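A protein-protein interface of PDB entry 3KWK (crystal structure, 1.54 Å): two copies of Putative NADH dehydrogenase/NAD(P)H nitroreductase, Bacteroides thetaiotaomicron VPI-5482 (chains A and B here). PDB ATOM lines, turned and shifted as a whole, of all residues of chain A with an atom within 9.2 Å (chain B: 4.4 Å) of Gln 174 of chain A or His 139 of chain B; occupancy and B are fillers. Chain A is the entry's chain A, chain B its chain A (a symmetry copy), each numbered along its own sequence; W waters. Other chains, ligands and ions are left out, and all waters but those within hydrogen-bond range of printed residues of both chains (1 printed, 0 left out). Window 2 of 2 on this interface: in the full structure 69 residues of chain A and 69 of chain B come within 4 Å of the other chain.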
ATOM      1  N   LYS A 168       1.622 -16.349  32.386  1.00  0.00           N
ATOM      2  CA  LYS A 168       1.453 -17.607  33.102  1.00  0.00           C
ATOM      3  C   LYS A 168       0.833 -18.694  32.222  1.00  0.00           C
ATOM      4  O   LYS A 168       0.929 -19.874  32.541  1.00  0.00           O
ATOM      5  CB  LYS A 168       0.579 -17.420  34.351  1.00  0.00           C
ATOM      6  CG  LYS A 168       1.083 -16.377  35.339  1.00  0.00           C
ATOM      7  CD  LYS A 168       0.262 -16.363  36.619  1.00  0.00           C
ATOM      8  CE  LYS A 168      -1.170 -15.956  36.374  1.00  0.00           C
ATOM      9  NZ  LYS A 168      -1.260 -14.604  35.765  1.00  0.00           N
ATOM     10  N   ILE A 170       1.756 -19.304  29.122  1.00  0.00           N
ATOM     11  CA  ILE A 170       2.772 -19.759  28.169  1.00  0.00           C
ATOM     12  C   ILE A 170       3.679 -20.767  28.852  1.00  0.00           C
ATOM     13  O   ILE A 170       4.210 -20.489  29.932  1.00  0.00           O
ATOM     14  CB  ILE A 170       3.608 -18.607  27.604  1.00  0.00           C
ATOM     15  CG1 ILE A 170       2.664 -17.608  26.906  1.00  0.00           C
ATOM     16  CG2 ILE A 170       4.699 -19.137  26.641  1.00  0.00           C
ATOM     17  CD1 ILE A 170       3.301 -16.284  26.601  1.00  0.00           C
ATOM     18  N   HIS A 171       3.823 -21.933  28.226  1.00  0.00           N
ATOM     19  CA  HIS A 171       4.617 -23.052  28.722  1.00  0.00           C
ATOM     20  C   HIS A 171       5.618 -23.413  27.625  1.00  0.00           C
ATOM     21  O   HIS A 171       5.263 -23.458  26.474  1.00  0.00           O
ATOM     22  CB  HIS A 171       3.721 -24.246  29.073  1.00  0.00           C
ATOM     23  CG  HIS A 171       2.560 -23.880  29.953  1.00  0.00           C
ATOM     24  ND1 HIS A 171       2.559 -24.070  31.321  1.00  0.00           N
ATOM     25  CD2 HIS A 171       1.379 -23.282  29.659  1.00  0.00           C
ATOM     26  CE1 HIS A 171       1.414 -23.630  31.819  1.00  0.00           C
ATOM     27  NE2 HIS A 171       0.691 -23.119  30.843  1.00  0.00           N
ATOM     28  N   TYR A 172       6.885 -23.569  27.976  1.00  0.00           N
ATOM     29  CA  TYR A 172       7.899 -24.005  27.017  1.00  0.00           C
ATOM     30  C   TYR A 172       8.205 -25.496  27.155  1.00  0.00           C
ATOM     31  O   TYR A 172       8.731 -25.956  28.179  1.00  0.00           O
ATOM     32  CB  TYR A 172       9.147 -23.151  27.204  1.00  0.00           C
ATOM     33  CG  TYR A 172       8.889 -21.724  26.830  1.00  0.00           C
ATOM     34  CD1 TYR A 172       8.802 -21.368  25.493  1.00  0.00           C
ATOM     35  CD2 TYR A 172       8.672 -20.734  27.785  1.00  0.00           C
ATOM     36  CE1 TYR A 172       8.515 -20.060  25.108  1.00  0.00           C
ATOM     37  CE2 TYR A 172       8.404 -19.410  27.405  1.00  0.00           C
ATOM     38  CZ  TYR A 172       8.315 -19.089  26.067  1.00  0.00           C
ATOM     39  OH  TYR A 172       8.054 -17.786  25.642  1.00  0.00           O
ATOM     40  N   ASN A 173       7.872 -26.262  26.098  1.00  0.00           N
ATOM     41  CA  ASN A 173       8.161 -27.684  25.884  1.00  0.00           C
ATOM     42  C   ASN A 173       7.372 -28.630  26.756  1.00  0.00           C
ATOM     43  O   ASN A 173       6.940 -29.664  26.276  1.00  0.00           O
ATOM     44  CB  ASN A 173       9.667 -28.023  25.949  1.00  0.00           C
ATOM     45  CG  ASN A 173      10.445 -27.479  24.735  1.00  0.00           C
ATOM     46  OD1 ASN A 173      10.008 -27.646  23.604  1.00  0.00           O
ATOM     47  ND2 ASN A 173      11.583 -26.830  24.975  1.00  0.00           N
ATOM     48  N   GLN A 174       7.203 -28.276  28.024  1.00  0.00           N
ATOM     49  CA  GLN A 174       6.369 -29.057  28.954  1.00  0.00           C
ATOM     50  C   GLN A 174       5.673 -28.085  29.941  1.00  0.00           C
ATOM     51  O   GLN A 174       6.118 -26.959  30.146  1.00  0.00           O
ATOM     52  CB  GLN A 174       7.171 -30.154  29.611  1.00  0.00           C
ATOM     53  CG  GLN A 174       7.851 -29.798  30.837  1.00  0.00           C
ATOM     54  CD  GLN A 174       8.296 -31.049  31.608  1.00  0.00           C
ATOM     55  OE1 GLN A 174       7.853 -31.328  32.766  1.00  0.00           O
ATOM     56  NE2 GLN A 174       9.181 -31.831  30.955  1.00  0.00           N
ATOM     57  N   TYR A 175       4.554 -28.535  30.496  1.00  0.00           N
ATOM     58  CA  TYR A 175       3.662 -27.706  31.282  1.00  0.00           C
ATOM     59  C   TYR A 175       4.270 -26.996  32.505  1.00  0.00           C
ATOM     60  O   TYR A 175       4.880 -27.716  33.280  1.00  0.00           O
ATOM     61  CB  TYR A 175       2.476 -28.546  31.740  1.00  0.00           C
ATOM     62  CG  TYR A 175       1.279 -27.654  32.001  1.00  0.00           C
ATOM     63  CD1 TYR A 175       0.541 -27.121  30.936  1.00  0.00           C
ATOM     64  CD2 TYR A 175       0.896 -27.310  33.289  1.00  0.00           C
ATOM     65  CE1 TYR A 175      -0.533 -26.314  31.167  1.00  0.00           C
ATOM     66  CE2 TYR A 175      -0.222 -26.496  33.498  1.00  0.00           C
ATOM     67  CZ  TYR A 175      -0.902 -25.993  32.446  1.00  0.00           C
ATOM     68  OH  TYR A 175      -2.005 -25.191  32.656  1.00  0.00           O
ATOM     69  OXT TYR A 175       4.130 -25.757  32.749  1.00  0.00           O
ATOM     70  N   VAL B  57       1.409 -24.388  24.864  1.00  0.00           N
ATOM     71  CA  VAL B  57       2.732 -25.026  25.017  1.00  0.00           C
ATOM     72  C   VAL B  57       3.482 -24.732  23.720  1.00  0.00           C
ATOM     73  O   VAL B  57       3.077 -25.148  22.654  1.00  0.00           O
ATOM     74  CB  VAL B  57       2.671 -26.523  25.311  1.00  0.00           C
ATOM     75  CG1 VAL B  57       4.061 -27.139  25.566  1.00  0.00           C
ATOM     76  CG2 VAL B  57       1.741 -26.834  26.493  1.00  0.00           C
ATOM     77  N   ARG B 135      -0.481 -35.161  25.567  1.00  0.00           N
ATOM     78  CA  ARG B 135      -0.369 -35.148  27.038  1.00  0.00           C
ATOM     79  C   ARG B 135       0.929 -35.785  27.494  1.00  0.00           C
ATOM     80  O   ARG B 135       1.636 -35.268  28.365  1.00  0.00           O
ATOM     81  CB  ARG B 135      -1.561 -35.873  27.653  1.00  0.00           C
ATOM     82  CG  ARG B 135      -1.500 -35.993  29.175  1.00  0.00           C
ATOM     83  CD  ARG B 135      -2.803 -36.575  29.755  1.00  0.00           C
ATOM     84  NE  ARG B 135      -4.023 -35.975  29.122  1.00  0.00           N
ATOM     85  CZ  ARG B 135      -4.444 -34.715  29.307  1.00  0.00           C
ATOM     86  NH1 ARG B 135      -3.846 -33.899  30.143  1.00  0.00           N
ATOM     87  NH2 ARG B 135      -5.524 -34.292  28.695  1.00  0.00           N
ATOM     88  N   LYS B 136       1.308 -36.888  26.849  1.00  0.00           N
ATOM     89  CA  LYS B 136       2.489 -37.648  27.225  1.00  0.00           C
ATOM     90  C   LYS B 136       3.736 -36.778  27.019  1.00  0.00           C
ATOM     91  O   LYS B 136       4.596 -36.729  27.883  1.00  0.00           O
ATOM     92  CB  LYS B 136       2.550 -38.978  26.439  1.00  0.00           C
ATOM     93  CG  LYS B 136       3.867 -39.743  26.564  1.00  0.00           C
ATOM     94  CD  LYS B 136       4.026 -40.842  25.510  1.00  0.00           C
ATOM     95  CE  LYS B 136       5.283 -41.669  25.792  1.00  0.00           C
ATOM     96  NZ  LYS B 136       5.209 -42.979  25.138  1.00  0.00           N
ATOM     97  N   TYR B 137       3.861 -36.126  25.869  1.00  0.00           N
ATOM     98  CA  TYR B 137       5.094 -35.451  25.501  1.00  0.00           C
ATOM     99  C   TYR B 137       5.221 -34.069  26.118  1.00  0.00           C
ATOM    100  O   TYR B 137       6.335 -33.559  26.311  1.00  0.00           O
ATOM    101  CB  TYR B 137       5.256 -35.430  23.964  1.00  0.00           C
ATOM    102  CG  TYR B 137       5.662 -36.789  23.487  1.00  0.00           C
ATOM    103  CD1 TYR B 137       6.940 -37.271  23.752  1.00  0.00           C
ATOM    104  CD2 TYR B 137       4.762 -37.627  22.895  1.00  0.00           C
ATOM    105  CE1 TYR B 137       7.312 -38.563  23.379  1.00  0.00           C
ATOM    106  CE2 TYR B 137       5.127 -38.937  22.500  1.00  0.00           C
ATOM    107  CZ  TYR B 137       6.395 -39.378  22.760  1.00  0.00           C
ATOM    108  OH  TYR B 137       6.791 -40.661  22.378  1.00  0.00           O
ATOM    109  N   THR B 138       4.101 -33.473  26.483  1.00  0.00           N
ATOM    110  CA  THR B 138       4.129 -32.128  27.086  1.00  0.00           C
ATOM    111  C   THR B 138       3.740 -32.105  28.576  1.00  0.00           C
ATOM    112  O   THR B 138       3.716 -31.041  29.173  1.00  0.00           O
ATOM    113  CB  THR B 138       3.331 -31.092  26.279  1.00  0.00           C
ATOM    114  OG1 THR B 138       1.926 -31.417  26.227  1.00  0.00           O
ATOM    115  CG2 THR B 138       3.919 -30.981  24.897  1.00  0.00           C
ATOM    116  N   HIS B 139       3.474 -33.264  29.161  1.00  0.00           N
ATOM    117  CA  HIS B 139       3.242 -33.421  30.594  1.00  0.00           C
ATOM    118  C   HIS B 139       2.011 -32.633  31.064  1.00  0.00           C
ATOM    119  O   HIS B 139       2.017 -31.969  32.115  1.00  0.00           O
ATOM    120  CB  HIS B 139       4.479 -33.034  31.433  1.00  0.00           C
ATOM    121  CG  HIS B 139       5.690 -33.850  31.126  1.00  0.00           C
ATOM    122  ND1 HIS B 139       6.282 -34.672  32.056  1.00  0.00           N
ATOM    123  CD2 HIS B 139       6.389 -34.000  29.981  1.00  0.00           C
ATOM    124  CE1 HIS B 139       7.315 -35.279  31.496  1.00  0.00           C
ATOM    125  NE2 HIS B 139       7.395 -34.894  30.233  1.00  0.00           N
ATOM    126  N   LEU B 140       0.952 -32.684  30.288  1.00  0.00           N
ATOM    127  CA  LEU B 140      -0.242 -31.915  30.613  1.00  0.00           C
ATOM    128  C   LEU B 140      -0.973 -32.519  31.805  1.00  0.00           C
ATOM    129  O   LEU B 140      -1.223 -33.739  31.856  1.00  0.00           O
ATOM    130  CB  LEU B 140      -1.212 -31.861  29.436  1.00  0.00           C
ATOM    131  CG  LEU B 140      -0.715 -31.252  28.127  1.00  0.00           C
ATOM    132  CD1 LEU B 140      -1.853 -31.354  27.101  1.00  0.00           C
ATOM    133  CD2 LEU B 140      -0.227 -29.822  28.324  1.00  0.00           C
ATOM    134  N   PRO B 141      -1.261 -31.674  32.822  1.00  0.00           N
ATOM    135  CA  PRO B 141      -2.184 -32.136  33.847  1.00  0.00           C
ATOM    136  C   PRO B 141      -3.507 -32.622  33.259  1.00  0.00           C
ATOM    137  O   PRO B 141      -3.872 -32.187  32.185  1.00  0.00           O
ATOM    138  CB  PRO B 141      -2.367 -30.905  34.721  1.00  0.00           C
ATOM    139  CG  PRO B 141      -1.082 -30.036  34.516  1.00  0.00           C
ATOM    140  CD  PRO B 141      -0.838 -30.265  33.023  1.00  0.00           C
HETATM  141  O   HOH W   1       9.680 -33.565  28.667  1.00  0.00           O
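The backbone NH of Tyr 175 of chain A sits at hydrogen-bond distance from the backbone carbonyl oxygen of Thr 138 of chain B, 3.0 Å away.
No position is printed for both chains.
Of the 10 pairs that touch across the chains among the printed residues, none has its exchanged pair printed and touching as well.
The backbone carbonyl oxygen (O) of Pro 141 of chain B sits at hydrogen-bond distance from the guanidinium group (NH1) of Arg 135 of chain B.
OXT of Tyr 175 of chain A lies within hydrogen-bond range of ND1 of His 171 of chain A (2.7 Å).
NH1 of Arg 135 of chain B is in hydrogen-bond range of O of Leu 140 of chain B.
Water W1 bridges NE2 of Gln 174 of chain A (2.9 Å) and NE2 of His 139 of chain B (3.1 Å).
Of the 7 printed residues of chain A, 4 touch a printed residue of chain B.
Of the 8 printed residues of chain B, 6 touch a printed residue of chain A.
Hydrophobic or aromatic side chains of chain B that line the printed part of chain A: Val 57, His 139, Leu 140 and Pro 141.
Among the printed residues, 10 pairs touch across the chains.
Among the printed residues, no Asp or Glu carboxylate lies within 4 Å of a Lys or Arg side-chain nitrogen of the other chain.
CA of Val 57 of chain B touches O of His 171 of chain A, at 3.3 Å.
Asn 173 of chain A touches Val 57 of chain B.
Asn 173 of chain A touches Tyr 137 of chain B.
Asn 173 of chain A touches Thr 138 of chain B (O to CG2, 3.6 Å).
Gln 174 of chain A touches Thr 138 of chain B.
His 139 of chain B touches Gln 174 of chain A (NE2 to NE2, 3.6 Å).
Tyr 175 of chain A touches His 139 of chain B (CB to O, 3.5 Å).
Tyr 175 of chain A touches Leu 140 of chain B.
Tyr 175 of chain A touches Pro 141 of chain B (CD2 to CD, 3.4 Å).
Printed residues of chain B within 4 Å of His 171 of chain A: Val 57.
Printed residues of chain B within 4 Å of Asn 173 of chain A: Val 57 (3.8 Å), Tyr 137 (3.9 Å) and Thr 138 (3.6 Å).
Gln 174 of chain A touches just these residues of chain B: Thr 138 and His 139.
Of the printed residues of chain A, Thr 138 of chain B touches Asn 173 (3.6 Å), Gln 174 (3.3 Å) and Tyr 175 (3.0 Å).
Of chain A, only Gln 174 (3.6 Å) and Tyr 175 (3.5 Å) come within 4 Å of His 139 of chain B.
Printed residues of chain A within 4 Å of Leu 140 of chain B: Tyr 175.
The nearest residue of chain A that does not touch His 139 of chain B is Asn 173 of chain A (5.7 Å).
The nearest printed residue of chain A that does not touch Leu 140 of chain B is Gln 174 of chain A (6.4 Å).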
